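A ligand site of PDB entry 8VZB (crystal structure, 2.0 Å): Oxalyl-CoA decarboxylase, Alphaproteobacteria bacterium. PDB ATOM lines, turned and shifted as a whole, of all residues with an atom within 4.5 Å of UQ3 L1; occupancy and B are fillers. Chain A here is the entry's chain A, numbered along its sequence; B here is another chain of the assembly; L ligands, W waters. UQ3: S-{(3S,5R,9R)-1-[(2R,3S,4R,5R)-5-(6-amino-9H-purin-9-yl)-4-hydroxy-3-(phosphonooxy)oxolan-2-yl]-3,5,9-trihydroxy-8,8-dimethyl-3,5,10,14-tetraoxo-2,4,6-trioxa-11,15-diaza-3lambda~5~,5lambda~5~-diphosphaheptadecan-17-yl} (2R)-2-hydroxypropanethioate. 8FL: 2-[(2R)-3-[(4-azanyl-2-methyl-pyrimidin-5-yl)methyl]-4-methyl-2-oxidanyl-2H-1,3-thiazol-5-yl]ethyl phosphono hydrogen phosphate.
NH1 of Arg 406 lies within salt-bridge range of OD1 of Asp 403.
The guanidinium group (NH1) of Arg 266 sits at hydrogen-bond distance from a ring nitrogen (NE2) of His 288 (3.0 Å).
The side-chain amide oxygen (OD1) of Asn 360 lies within hydrogen-bond range of the side-chain amino group (NZ) of Lys 552 (3.4 Å).
The side-chain sulfur (SD) of Met 402 sits close to the backbone NH (N) of Ala 420.
The side-chain amide nitrogen (ND2) of Asn 360 sits at hydrogen-bond distance from the backbone carbonyl oxygen (O) of Gly 264, 2.6 Å away.
The guanidinium group (NH2) of Arg 266 sits at hydrogen-bond distance from the backbone carbonyl oxygen (O) of Ile 286 (2.9 Å).
Water W11 lies within hydrogen-bond range of an oxygen (O27) of UQ3 L1 and the backbone carbonyl oxygen of Gly 263.
Water W2 bridges O24 of UQ3 L1 and NH1 of Arg 266.
Water W4 lies within hydrogen-bond range of O51 of UQ3 L1 (2.7 Å) and OD1 of Asn 360 (2.7 Å).
Water W1 lies within hydrogen-bond range of an oxygen (O28) of UQ3 L1 (2.8 Å) and the backbone carbonyl oxygen (O) of Asp 403 (2.8 Å).
Water W7 bridges the side-chain amide oxygen of Gln 554 and an oxygen (O23) of UQ3 L1.
Water W9 bridges O49 of UQ3 L1 (3.0 Å) and OG of Ser 267 (3.2 Å).
Pro 248 touches UQ3 L1.
Ala 265 touches UQ3 L1 (N to O46, 3.5 Å).
Trp 285 touches UQ3 L1 (CZ3 to C18, 3.7 Å).
Ile 286 touches UQ3 L1 (O to C19, 3.2 Å).
His 288 touches UQ3 L1.
CG2 of Val 364 touches C42 of UQ3 L1, 3.8 Å away.
CB of Ala 399 touches C01 of UQ3 L1 (3.6 Å).
Met 402 touches UQ3 L1 (CE to O10, 3.8 Å).
CG2 of Thr 407 touches O29 of UQ3 L1, at 3.4 Å.
Gly 424 touches UQ3 L1.
Trp 558 touches UQ3 L1.
CA of Gly 37 of chain B touches O53 of UQ3 L1, at 3.7 Å.
Phe 122 of chain B touches UQ3 L1.
Hydrophobic or aromatic side chains within 4 Å of UQ3 L1: Pro 248, Trp 285, His 288, Val 364, Ala 399, Met 402, Trp 558, Phe 38 of chain B and Phe 122 of chain B.
Of the 28 residues printed, 23 come within 4 Å of UQ3 L1.
The nearest printed residue that does not touch UQ3 L1 is Gln 361 (4.02 Å).
An oxygen (O04) of UQ3 L1 lies close to an oxygen (OC2) of 8FL L2.
The side-chain carboxylate of Asp 403 is in hydrogen-bond range of a nitrogen (N13) of UQ3 L1 (3.2 Å).
An oxygen (O46) of UQ3 L1 lies within hydrogen-bond range of the side-chain amide nitrogen (ND2) of Asn 360, 3.3 Å away.
The backbone NH of Arg 266 is in hydrogen-bond range of an oxygen (O46) of UQ3 L1, at 3.1 Å.
The backbone NH of Ala 399 lies close to an oxygen (O1B) of 8FL L2 (3.4 Å).
An oxygen (O28) of UQ3 L1 lies within salt-bridge range of the guanidinium group of Arg 406, 2.7 Å away.
An oxygen (O46) of UQ3 L1 lies close to the backbone carbonyl oxygen (O) of Gly 264 (3.3 Å).
N of Phe 38 of chain B is in hydrogen-bond range of O04 of UQ3 L1 (3.4 Å).
The side-chain amino group of Lys 552 lies within salt-bridge range of an oxygen (O51) of UQ3 L1, 3.1 Å away.
An oxygen (O46) of UQ3 L1 lies close to the backbone carbonyl oxygen (O) of Gly 263, at 3.3 Å.
The side-chain amide nitrogen (NE2) of Gln 554 is in hydrogen-bond range of an oxygen (O49) of UQ3 L1.
The guanidinium group of Arg 266 is in salt-bridge range of an oxygen (O24) of UQ3 L1 (3.5 Å).
A nitrogen (N4') of 8FL L2 sits at hydrogen-bond distance from the backbone carbonyl oxygen of Gly 424.
N of Ser 267 is in hydrogen-bond range of O50 of UQ3 L1 (2.9 Å).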
ATOM      1  N   PRO A 248     -14.487  12.793   2.059  1.00  0.00           N
ATOM      2  CA  PRO A 248     -13.542  13.385   3.017  1.00  0.00           C
ATOM      3  C   PRO A 248     -12.856  14.656   2.540  1.00  0.00           C
ATOM      4  O   PRO A 248     -12.953  15.690   3.206  1.00  0.00           O
ATOM      5  CB  PRO A 248     -12.541  12.253   3.254  1.00  0.00           C
ATOM      6  CG  PRO A 248     -13.395  11.036   3.166  1.00  0.00           C
ATOM      7  CD  PRO A 248     -14.418  11.318   2.081  1.00  0.00           C
ATOM      8  N   GLY A 263     -24.330  15.049   5.664  1.00  0.00           N
ATOM      9  CA  GLY A 263     -23.150  14.495   6.294  1.00  0.00           C
ATOM     10  C   GLY A 263     -23.447  13.808   7.619  1.00  0.00           C
ATOM     11  O   GLY A 263     -22.849  12.777   7.938  1.00  0.00           O
ATOM     12  N   GLY A 264     -24.369  14.367   8.401  1.00  0.00           N
ATOM     13  CA  GLY A 264     -24.742  13.792   9.676  1.00  0.00           C
ATOM     14  C   GLY A 264     -25.689  12.620   9.600  1.00  0.00           C
ATOM     15  O   GLY A 264     -26.110  12.094  10.633  1.00  0.00           O
ATOM     16  N   ALA A 265     -26.069  12.199   8.388  1.00  0.00           N
ATOM     17  CA  ALA A 265     -26.904  11.027   8.159  1.00  0.00           C
ATOM     18  C   ALA A 265     -26.326  10.206   7.019  1.00  0.00           C
ATOM     19  O   ALA A 265     -27.045   9.717   6.144  1.00  0.00           O
ATOM     20  CB  ALA A 265     -28.350  11.429   7.859  1.00  0.00           C
ATOM     21  N   ARG A 266     -24.999  10.035   7.016  1.00  0.00           N
ATOM     22  CA  ARG A 266     -24.300   9.516   5.848  1.00  0.00           C
ATOM     23  C   ARG A 266     -24.704   8.084   5.539  1.00  0.00           C
ATOM     24  O   ARG A 266     -25.018   7.746   4.386  1.00  0.00           O
ATOM     25  CB  ARG A 266     -22.788   9.626   6.048  1.00  0.00           C
ATOM     26  CG  ARG A 266     -21.963   9.011   4.913  1.00  0.00           C
ATOM     27  CD  ARG A 266     -20.479   9.187   5.167  1.00  0.00           C
ATOM     28  NE  ARG A 266     -19.659   8.731   4.042  1.00  0.00           N
ATOM     29  CZ  ARG A 266     -19.274   7.473   3.860  1.00  0.00           C
ATOM     30  NH1 ARG A 266     -19.618   6.514   4.691  1.00  0.00           N
ATOM     31  NH2 ARG A 266     -18.525   7.187   2.801  1.00  0.00           N
ATOM     32  N   SER A 267     -24.718   7.214   6.548  1.00  0.00           N
ATOM     33  CA  SER A 267     -25.001   5.804   6.297  1.00  0.00           C
ATOM     34  C   SER A 267     -26.419   5.610   5.793  1.00  0.00           C
ATOM     35  O   SER A 267     -26.652   4.800   4.883  1.00  0.00           O
ATOM     36  CB  SER A 267     -24.754   4.988   7.559  1.00  0.00           C
ATOM     37  OG  SER A 267     -24.774   3.604   7.266  1.00  0.00           O
ATOM     38  N   HIS A 268     -27.385   6.342   6.353  1.00  0.00           N
ATOM     39  CA  HIS A 268     -28.762   6.222   5.876  1.00  0.00           C
ATOM     40  C   HIS A 268     -28.896   6.713   4.438  1.00  0.00           C
ATOM     41  O   HIS A 268     -29.611   6.105   3.631  1.00  0.00           O
ATOM     42  CB  HIS A 268     -29.708   6.993   6.786  1.00  0.00           C
ATOM     43  CG  HIS A 268     -31.140   6.924   6.345  1.00  0.00           C
ATOM     44  ND1 HIS A 268     -31.984   5.916   6.743  1.00  0.00           N
ATOM     45  CD2 HIS A 268     -31.866   7.725   5.537  1.00  0.00           C
ATOM     46  CE1 HIS A 268     -33.175   6.104   6.203  1.00  0.00           C
ATOM     47  NE2 HIS A 268     -33.134   7.195   5.465  1.00  0.00           N
ATOM     48  N   TRP A 285     -13.156   2.208  -2.095  1.00  0.00           N
ATOM     49  CA  TRP A 285     -13.435   1.895  -0.692  1.00  0.00           C
ATOM     50  C   TRP A 285     -13.998   3.094   0.071  1.00  0.00           C
ATOM     51  O   TRP A 285     -14.770   2.922   1.018  1.00  0.00           O
ATOM     52  CB  TRP A 285     -12.178   1.380  -0.005  1.00  0.00           C
ATOM     53  CG  TRP A 285     -11.077   2.395   0.084  1.00  0.00           C
ATOM     54  CD1 TRP A 285     -10.127   2.656  -0.854  1.00  0.00           C
ATOM     55  CD2 TRP A 285     -10.813   3.272   1.187  1.00  0.00           C
ATOM     56  NE1 TRP A 285      -9.287   3.657  -0.417  1.00  0.00           N
ATOM     57  CE2 TRP A 285      -9.687   4.053   0.831  1.00  0.00           C
ATOM     58  CE3 TRP A 285     -11.419   3.494   2.426  1.00  0.00           C
ATOM     59  CZ2 TRP A 285      -9.159   5.021   1.679  1.00  0.00           C
ATOM     60  CZ3 TRP A 285     -10.889   4.454   3.263  1.00  0.00           C
ATOM     61  CH2 TRP A 285      -9.768   5.211   2.889  1.00  0.00           C
ATOM     62  N   ILE A 286     -13.639   4.318  -0.328  1.00  0.00           N
ATOM     63  CA  ILE A 286     -14.113   5.486   0.413  1.00  0.00           C
ATOM     64  C   ILE A 286     -15.631   5.649   0.268  1.00  0.00           C
ATOM     65  O   ILE A 286     -16.302   6.119   1.198  1.00  0.00           O
ATOM     66  CB  ILE A 286     -13.344   6.748  -0.040  1.00  0.00           C
ATOM     67  CG1 ILE A 286     -12.043   6.882   0.763  1.00  0.00           C
ATOM     68  CG2 ILE A 286     -14.172   8.022   0.106  1.00  0.00           C
ATOM     69  CD1 ILE A 286     -11.215   8.100   0.432  1.00  0.00           C
ATOM     70  N   HIS A 288     -17.494   2.827  -0.481  1.00  0.00           N
ATOM     71  CA  HIS A 288     -17.998   1.472  -0.265  1.00  0.00           C
ATOM     72  C   HIS A 288     -18.487   0.832  -1.567  1.00  0.00           C
ATOM     73  O   HIS A 288     -19.458   0.084  -1.583  1.00  0.00           O
ATOM     74  CB  HIS A 288     -19.087   1.466   0.802  1.00  0.00           C
ATOM     75  CG  HIS A 288     -18.776   2.329   1.984  1.00  0.00           C
ATOM     76  ND1 HIS A 288     -17.790   2.020   2.898  1.00  0.00           N
ATOM     77  CD2 HIS A 288     -19.298   3.511   2.384  1.00  0.00           C
ATOM     78  CE1 HIS A 288     -17.731   2.969   3.807  1.00  0.00           C
ATOM     79  NE2 HIS A 288     -18.632   3.882   3.527  1.00  0.00           N
ATOM     80  N   ASN A 360     -28.180  11.260  15.131  1.00  0.00           N
ATOM     81  CA  ASN A 360     -26.740  11.180  15.275  1.00  0.00           C
ATOM     82  C   ASN A 360     -26.203  12.334  16.123  1.00  0.00           C
ATOM     83  O   ASN A 360     -25.250  12.157  16.893  1.00  0.00           O
ATOM     84  CB  ASN A 360     -26.062  11.151  13.909  1.00  0.00           C
ATOM     85  CG  ASN A 360     -26.163   9.798  13.223  1.00  0.00           C
ATOM     86  OD1 ASN A 360     -26.257   8.765  13.893  1.00  0.00           O
ATOM     87  ND2 ASN A 360     -26.148   9.803  11.903  1.00  0.00           N
ATOM     88  N   GLN A 361     -26.813  13.520  15.988  1.00  0.00           N
ATOM     89  CA  GLN A 361     -26.434  14.648  16.832  1.00  0.00           C
ATOM     90  C   GLN A 361     -26.657  14.342  18.307  1.00  0.00           C
ATOM     91  O   GLN A 361     -25.789  14.580  19.149  1.00  0.00           O
ATOM     92  CB  GLN A 361     -27.196  15.906  16.419  1.00  0.00           C
ATOM     93  CG  GLN A 361     -26.730  16.520  15.112  1.00  0.00           C
ATOM     94  CD  GLN A 361     -27.630  17.643  14.639  1.00  0.00           C
ATOM     95  OE1 GLN A 361     -28.738  17.826  15.149  1.00  0.00           O
ATOM     96  NE2 GLN A 361     -27.158  18.408  13.656  1.00  0.00           N
ATOM     97  N   VAL A 364     -24.008  11.817  19.851  1.00  0.00           N
ATOM     98  CA  VAL A 364     -22.687  12.312  20.218  1.00  0.00           C
ATOM     99  C   VAL A 364     -22.731  13.508  21.157  1.00  0.00           C
ATOM    100  O   VAL A 364     -21.686  13.869  21.721  1.00  0.00           O
ATOM    101  CB  VAL A 364     -21.860  12.689  18.969  1.00  0.00           C
ATOM    102  CG1 VAL A 364     -21.627  11.460  18.090  1.00  0.00           C
ATOM    103  CG2 VAL A 364     -22.551  13.791  18.180  1.00  0.00           C
ATOM    104  N   GLY A 398      -4.299  10.150  11.185  1.00  0.00           N
ATOM    105  CA  GLY A 398      -4.473   9.166  12.224  1.00  0.00           C
ATOM    106  C   GLY A 398      -5.640   8.270  11.872  1.00  0.00           C
ATOM    107  O   GLY A 398      -6.141   8.270  10.750  1.00  0.00           O
ATOM    108  N   ALA A 399      -6.078   7.480  12.850  1.00  0.00           N
ATOM    109  CA  ALA A 399      -7.269   6.658  12.664  1.00  0.00           C
ATOM    110  C   ALA A 399      -8.460   7.346  13.327  1.00  0.00           C
ATOM    111  O   ALA A 399      -9.245   8.013  12.656  1.00  0.00           O
ATOM    112  CB  ALA A 399      -7.066   5.245  13.201  1.00  0.00           C
ATOM    113  N   MET A 402      -8.228  11.249  13.054  1.00  0.00           N
ATOM    114  CA  MET A 402      -8.568  11.793  11.745  1.00  0.00           C
ATOM    115  C   MET A 402     -10.064  11.633  11.450  1.00  0.00           C
ATOM    116  O   MET A 402     -10.729  12.583  11.027  1.00  0.00           O
ATOM    117  CB  MET A 402      -7.742  11.113  10.661  1.00  0.00           C
ATOM    118  CG  MET A 402      -7.878  11.735   9.291  1.00  0.00           C
ATOM    119  SD  MET A 402      -6.845  10.875   8.081  1.00  0.00           S
ATOM    120  CE  MET A 402      -7.740   9.321   7.958  1.00  0.00           C
ATOM    121  N   ASP A 403     -10.598  10.433  11.678  1.00  0.00           N
ATOM    122  CA  ASP A 403     -11.981  10.167  11.288  1.00  0.00           C
ATOM    123  C   ASP A 403     -12.960  10.992  12.107  1.00  0.00           C
ATOM    124  O   ASP A 403     -13.930  11.537  11.559  1.00  0.00           O
ATOM    125  CB  ASP A 403     -12.288   8.666  11.412  1.00  0.00           C
ATOM    126  CG  ASP A 403     -11.570   7.824  10.347  1.00  0.00           C
ATOM    127  OD1 ASP A 403     -11.175   8.386   9.301  1.00  0.00           O
ATOM    128  OD2 ASP A 403     -11.413   6.605  10.547  1.00  0.00           O
ATOM    129  N   ARG A 406     -12.800  14.544  11.065  1.00  0.00           N
ATOM    130  CA  ARG A 406     -13.475  14.778   9.797  1.00  0.00           C
ATOM    131  C   ARG A 406     -14.901  15.276  10.002  1.00  0.00           C
ATOM    132  O   ARG A 406     -15.377  16.150   9.268  1.00  0.00           O
ATOM    133  CB  ARG A 406     -13.453  13.511   8.956  1.00  0.00           C
ATOM    134  CG  ARG A 406     -14.072  13.641   7.577  1.00  0.00           C
ATOM    135  CD  ARG A 406     -13.914  12.362   6.767  1.00  0.00           C
ATOM    136  NE  ARG A 406     -14.379  11.190   7.502  1.00  0.00           N
ATOM    137  CZ  ARG A 406     -13.589  10.213   7.941  1.00  0.00           C
ATOM    138  NH1 ARG A 406     -12.291  10.210   7.686  1.00  0.00           N
ATOM    139  NH2 ARG A 406     -14.128   9.213   8.642  1.00  0.00           N
ATOM    140  N   THR A 407     -15.604  14.720  10.997  1.00  0.00           N
ATOM    141  CA  THR A 407     -16.965  15.158  11.264  1.00  0.00           C
ATOM    142  C   THR A 407     -17.030  16.392  12.154  1.00  0.00           C
ATOM    143  O   THR A 407     -18.006  17.138  12.079  1.00  0.00           O
ATOM    144  CB  THR A 407     -17.783  14.033  11.911  1.00  0.00           C
ATOM    145  OG1 THR A 407     -17.297  13.783  13.237  1.00  0.00           O
ATOM    146  CG2 THR A 407     -17.677  12.756  11.094  1.00  0.00           C
ATOM    147  N   ALA A 420      -5.358  11.714   4.968  1.00  0.00           N
ATOM    148  CA  ALA A 420      -4.687  10.497   4.537  1.00  0.00           C
ATOM    149  C   ALA A 420      -5.065  10.072   3.131  1.00  0.00           C
ATOM    150  O   ALA A 420      -4.321   9.296   2.512  1.00  0.00           O
ATOM    151  CB  ALA A 420      -4.966   9.353   5.512  1.00  0.00           C
ATOM    152  N   GLY A 424      -4.899   5.963   2.286  1.00  0.00           N
ATOM    153  CA  GLY A 424      -4.869   5.764   3.727  1.00  0.00           C
ATOM    154  C   GLY A 424      -3.487   5.943   4.321  1.00  0.00           C
ATOM    155  O   GLY A 424      -3.083   5.165   5.198  1.00  0.00           O
ATOM    156  N   LYS A 552     -18.098   7.291  17.537  1.00  0.00           N
ATOM    157  CA  LYS A 552     -19.502   6.942  17.726  1.00  0.00           C
ATOM    158  C   LYS A 552     -19.779   5.562  17.126  1.00  0.00           C
ATOM    159  O   LYS A 552     -19.311   5.260  16.026  1.00  0.00           O
ATOM    160  CB  LYS A 552     -20.412   7.983  17.072  1.00  0.00           C
ATOM    161  CG  LYS A 552     -21.893   7.629  17.086  1.00  0.00           C
ATOM    162  CD  LYS A 552     -22.725   8.590  16.250  1.00  0.00           C
ATOM    163  CE  LYS A 552     -22.595   8.313  14.748  1.00  0.00           C
ATOM    164  NZ  LYS A 552     -23.305   7.066  14.345  1.00  0.00           N
ATOM    165  N   GLN A 554     -21.480   2.681  15.030  1.00  0.00           N
ATOM    166  CA  GLN A 554     -22.155   2.719  13.735  1.00  0.00           C
ATOM    167  C   GLN A 554     -22.669   1.332  13.390  1.00  0.00           C
ATOM    168  O   GLN A 554     -22.235   0.323  13.955  1.00  0.00           O
ATOM    169  CB  GLN A 554     -21.229   3.194  12.618  1.00  0.00           C
ATOM    170  CG  GLN A 554     -20.760   4.625  12.743  1.00  0.00           C
ATOM    171  CD  GLN A 554     -19.677   4.941  11.739  1.00  0.00           C
ATOM    172  OE1 GLN A 554     -18.491   4.738  12.010  1.00  0.00           O
ATOM    173  NE2 GLN A 554     -20.067   5.444  10.575  1.00  0.00           N
ATOM    174  N   TRP A 558     -16.106   1.005   8.984  1.00  0.00           N
ATOM    175  CA  TRP A 558     -15.689   1.857   7.873  1.00  0.00           C
ATOM    176  C   TRP A 558     -15.083   1.056   6.738  1.00  0.00           C
ATOM    177  O   TRP A 558     -15.222   1.426   5.566  1.00  0.00           O
ATOM    178  CB  TRP A 558     -14.701   2.926   8.361  1.00  0.00           C
ATOM    179  CG  TRP A 558     -13.350   2.409   8.769  1.00  0.00           C
ATOM    180  CD1 TRP A 558     -12.934   2.112  10.035  1.00  0.00           C
ATOM    181  CD2 TRP A 558     -12.235   2.134   7.899  1.00  0.00           C
ATOM    182  NE1 TRP A 558     -11.640   1.669  10.010  1.00  0.00           N
ATOM    183  CE2 TRP A 558     -11.186   1.670   8.715  1.00  0.00           C
ATOM    184  CE3 TRP A 558     -12.028   2.233   6.522  1.00  0.00           C
ATOM    185  CZ2 TRP A 558      -9.946   1.306   8.198  1.00  0.00           C
ATOM    186  CZ3 TRP A 558     -10.788   1.869   6.005  1.00  0.00           C
ATOM    187  CH2 TRP A 558      -9.765   1.418   6.845  1.00  0.00           C
ATOM    188  N   GLY B  37      -1.184  -2.312  11.873  1.00  0.00           N
ATOM    189  CA  GLY B  37      -2.292  -1.725  11.145  1.00  0.00           C
ATOM    190  C   GLY B  37      -2.907  -2.819  10.287  1.00  0.00           C
ATOM    191  O   GLY B  37      -2.408  -3.939  10.224  1.00  0.00           O
ATOM    192  N   PHE B  38      -4.012  -2.458   9.637  1.00  0.00           N
ATOM    193  CA  PHE B  38      -4.618  -3.378   8.689  1.00  0.00           C
ATOM    194  C   PHE B  38      -3.580  -3.727   7.617  1.00  0.00           C
ATOM    195  O   PHE B  38      -2.928  -2.824   7.094  1.00  0.00           O
ATOM    196  CB  PHE B  38      -5.863  -2.774   8.033  1.00  0.00           C
ATOM    197  CG  PHE B  38      -6.420  -3.606   6.912  1.00  0.00           C
ATOM    198  CD1 PHE B  38      -7.310  -4.630   7.166  1.00  0.00           C
ATOM    199  CD2 PHE B  38      -6.006  -3.389   5.606  1.00  0.00           C
ATOM    200  CE1 PHE B  38      -7.817  -5.412   6.127  1.00  0.00           C
ATOM    201  CE2 PHE B  38      -6.500  -4.158   4.559  1.00  0.00           C
ATOM    202  CZ  PHE B  38      -7.404  -5.172   4.831  1.00  0.00           C
ATOM    203  N   ILE B  41      -1.896  -6.698  11.941  1.00  0.00           N
ATOM    204  CA  ILE B  41      -1.967  -6.773  13.401  1.00  0.00           C
ATOM    205  C   ILE B  41      -1.935  -8.223  13.897  1.00  0.00           C
ATOM    206  O   ILE B  41      -1.173  -8.501  14.838  1.00  0.00           O
ATOM    207  CB  ILE B  41      -3.180  -5.990  13.907  1.00  0.00           C
ATOM    208  CG1 ILE B  41      -2.982  -4.497  13.670  1.00  0.00           C
ATOM    209  CG2 ILE B  41      -3.426  -6.274  15.380  1.00  0.00           C
ATOM    210  CD1 ILE B  41      -4.183  -3.659  14.016  1.00  0.00           C
ATOM    211  N   PHE B 122      -9.240  -0.688  -0.112  1.00  0.00           N
ATOM    212  CA  PHE B 122      -8.376   0.071   0.770  1.00  0.00           C
ATOM    213  C   PHE B 122      -6.935  -0.421   0.670  1.00  0.00           C
ATOM    214  O   PHE B 122      -6.643  -1.563   1.029  1.00  0.00           O
ATOM    215  CB  PHE B 122      -8.878  -0.022   2.213  1.00  0.00           C
ATOM    216  CG  PHE B 122      -7.993   0.652   3.219  1.00  0.00           C
ATOM    217  CD1 PHE B 122      -8.006   2.031   3.359  1.00  0.00           C
ATOM    218  CD2 PHE B 122      -7.148  -0.091   4.037  1.00  0.00           C
ATOM    219  CE1 PHE B 122      -7.200   2.657   4.286  1.00  0.00           C
ATOM    220  CE2 PHE B 122      -6.338   0.536   4.974  1.00  0.00           C
ATOM    221  CZ  PHE B 122      -6.367   1.907   5.100  1.00  0.00           C
HETATM  222  C17 UQ3 L   1     -15.014   6.390   5.096  1.00  0.00           C
HETATM  223  C20 UQ3 L   1     -16.300   5.912   5.758  1.00  0.00           C
HETATM  224  C01 UQ3 L   1      -7.105   1.618  12.805  1.00  0.00           C
HETATM  225  C02 UQ3 L   1      -5.820   1.388  12.033  1.00  0.00           C
HETATM  226  C03 UQ3 L   1      -6.084   1.489  10.556  1.00  0.00           C
HETATM  227  C06 UQ3 L   1      -6.532   3.110   8.443  1.00  0.00           C
HETATM  228  C07 UQ3 L   1      -6.608   4.626   8.306  1.00  0.00           C
HETATM  229  C09 UQ3 L   1      -8.376   5.527   6.852  1.00  0.00           C
HETATM  230  C11 UQ3 L   1      -9.877   5.515   6.738  1.00  0.00           C
HETATM  231  C12 UQ3 L   1     -10.442   6.879   6.413  1.00  0.00           C
HETATM  232  C14 UQ3 L   1     -12.747   7.274   5.768  1.00  0.00           C
HETATM  233  C16 UQ3 L   1     -14.182   7.098   6.160  1.00  0.00           C
HETATM  234  C18 UQ3 L   1     -14.268   5.179   4.532  1.00  0.00           C
HETATM  235  C19 UQ3 L   1     -15.360   7.360   3.974  1.00  0.00           C
HETATM  236  C30 UQ3 L   1     -19.165   9.035  10.691  1.00  0.00           C
HETATM  237  C31 UQ3 L   1     -20.529   8.988  11.386  1.00  0.00           C
HETATM  238  C32 UQ3 L   1     -21.666   8.756  10.414  1.00  0.00           C
HETATM  239  C33 UQ3 L   1     -22.214  10.142  10.146  1.00  0.00           C
HETATM  240  C34 UQ3 L   1     -22.016  10.807  11.500  1.00  0.00           C
HETATM  241  C37 UQ3 L   1     -21.271  12.995  10.487  1.00  0.00           C
HETATM  242  C39 UQ3 L   1     -21.901  14.379  12.054  1.00  0.00           C
HETATM  243  C40 UQ3 L   1     -22.209  15.431  12.911  1.00  0.00           C
HETATM  244  C42 UQ3 L   1     -23.130  13.910  14.430  1.00  0.00           C
HETATM  245  C44 UQ3 L   1     -22.231  13.093  12.432  1.00  0.00           C
HETATM  246  N08 UQ3 L   1      -7.974   4.860   7.912  1.00  0.00           N
HETATM  247  N13 UQ3 L   1     -11.867   6.800   6.631  1.00  0.00           N
HETATM  248  N36 UQ3 L   1     -21.850  12.271  11.455  1.00  0.00           N
HETATM  249  N38 UQ3 L   1     -21.309  14.305  10.841  1.00  0.00           N
HETATM  250  N41 UQ3 L   1     -22.817  15.173  14.087  1.00  0.00           N
HETATM  251  N43 UQ3 L   1     -22.850  12.873  13.621  1.00  0.00           N
HETATM  252  N45 UQ3 L   1     -21.891  16.709  12.575  1.00  0.00           N
HETATM  253  O04 UQ3 L   1      -5.549   0.598   9.721  1.00  0.00           O
HETATM  254  O10 UQ3 L   1      -7.629   6.049   6.042  1.00  0.00           O
HETATM  255  O15 UQ3 L   1     -12.407   7.828   4.741  1.00  0.00           O
HETATM  256  O21 UQ3 L   1     -17.033   7.055   6.196  1.00  0.00           O
HETATM  257  O23 UQ3 L   1     -16.497   7.147   8.693  1.00  0.00           O
HETATM  258  O24 UQ3 L   1     -18.545   5.966   7.933  1.00  0.00           O
HETATM  259  O25 UQ3 L   1     -18.529   8.479   7.759  1.00  0.00           O
HETATM  260  O27 UQ3 L   1     -18.431  10.982   7.438  1.00  0.00           O
HETATM  261  O28 UQ3 L   1     -16.721   9.926   8.929  1.00  0.00           O
HETATM  262  O29 UQ3 L   1     -19.129  10.056   9.701  1.00  0.00           O
HETATM  263  O35 UQ3 L   1     -20.804  10.243  12.022  1.00  0.00           O
HETATM  264  O46 UQ3 L   1     -23.589  10.107   9.773  1.00  0.00           O
HETATM  265  O47 UQ3 L   1     -22.623   8.001  11.144  1.00  0.00           O
HETATM  266  O49 UQ3 L   1     -22.776   5.832   9.851  1.00  0.00           O
HETATM  267  O50 UQ3 L   1     -24.414   7.651   9.419  1.00  0.00           O
HETATM  268  O51 UQ3 L   1     -24.504   6.373  11.538  1.00  0.00           O
HETATM  269  O52 UQ3 L   1     -14.240   6.329   7.365  1.00  0.00           O
HETATM  270  O53 UQ3 L   1      -5.311   0.084  12.359  1.00  0.00           O
HETATM  271  P22 UQ3 L   1     -17.631   7.146   7.684  1.00  0.00           P
HETATM  272  P26 UQ3 L   1     -18.146   9.886   8.446  1.00  0.00           P
HETATM  273  P48 UQ3 L   1     -23.598   6.934  10.467  1.00  0.00           P
HETATM  274  S05 UQ3 L   1      -7.025   2.677  10.019  1.00  0.00           S
HETATM  275  C4' 8FL L   2      -0.721   3.355   7.451  1.00  0.00           C
HETATM  276  C5' 8FL L   2      -0.282   2.599   8.558  1.00  0.00           C
HETATM  277  C6' 8FL L   2       1.089   2.463   8.677  1.00  0.00           C
HETATM  278  N1' 8FL L   2       1.963   2.995   7.798  1.00  0.00           N
HETATM  279  N3' 8FL L   2       0.154   3.901   6.570  1.00  0.00           N
HETATM  280  C2' 8FL L   2       1.449   3.702   6.759  1.00  0.00           C
HETATM  281  CM4 8FL L   2       0.033   3.417  11.978  1.00  0.00           C
HETATM  282  CM2 8FL L   2       2.408   4.301   5.782  1.00  0.00           C
HETATM  283  C7  8FL L   2      -3.334   5.431  14.101  1.00  0.00           C
HETATM  284  C6  8FL L   2      -2.091   5.412  13.239  1.00  0.00           C
HETATM  285  C7' 8FL L   2      -1.193   2.001   9.567  1.00  0.00           C
HETATM  286  C4  8FL L   2      -1.352   3.694  11.476  1.00  0.00           C
HETATM  287  C5  8FL L   2      -2.243   4.567  12.004  1.00  0.00           C
HETATM  288  C2  8FL L   2      -3.089   3.462  10.006  1.00  0.00           C
HETATM  289  N4' 8FL L   2      -2.025   3.577   7.208  1.00  0.00           N
HETATM  290  N3  8FL L   2      -1.865   3.037  10.348  1.00  0.00           N
HETATM  291  O3B 8FL L   2      -6.259   8.617  17.326  1.00  0.00           O
HETATM  292  O1A 8FL L   2      -2.266   7.663  17.073  1.00  0.00           O
HETATM  293  OC2 8FL L   2      -3.771   3.095   8.940  1.00  0.00           O
HETATM  294  O2B 8FL L   2      -4.790   6.661  17.932  1.00  0.00           O
HETATM  295  O1B 8FL L   2      -6.447   6.459  16.040  1.00  0.00           O
HETATM  296  O2A 8FL L   2      -2.212   8.257  14.588  1.00  0.00           O
HETATM  297  O7  8FL L   2      -2.982   5.971  15.396  1.00  0.00           O
HETATM  298  O3A 8FL L   2      -4.393   7.921  15.821  1.00  0.00           O
HETATM  299  PB  8FL L   2      -5.540   7.380  16.825  1.00  0.00           P
HETATM  300  PA  8FL L   2      -2.847   7.522  15.712  1.00  0.00           P
HETATM  301  S1  8FL L   2      -3.726   4.632  11.109  1.00  0.00           S
HETATM  302  O   HOH W   1     -15.966   9.600  11.612  1.00  0.00           O
HETATM  303  O   HOH W   2     -21.137   6.120   7.170  1.00  0.00           O
HETATM  304  O   HOH W   3      -7.858   8.179   4.305  1.00  0.00           O
HETATM  305  O   HOH W   4     -27.064   6.539  12.502  1.00  0.00           O
HETATM  306  O   HOH W   5     -27.038   7.544   8.770  1.00  0.00           O
HETATM  307  O   HOH W   6     -25.035   3.835  11.502  1.00  0.00           O
HETATM  308  O   HOH W   7     -16.220   5.292  10.786  1.00  0.00           O
HETATM  309  O   HOH W   8     -10.312   9.449   4.084  1.00  0.00           O
HETATM  310  O   HOH W   9     -22.443   2.895   9.390  1.00  0.00           O
HETATM  311  O   HOH W  10     -18.981   3.286   8.008  1.00  0.00           O
HETATM  312  O   HOH W  11     -20.203  12.540   6.604  1.00  0.00           O
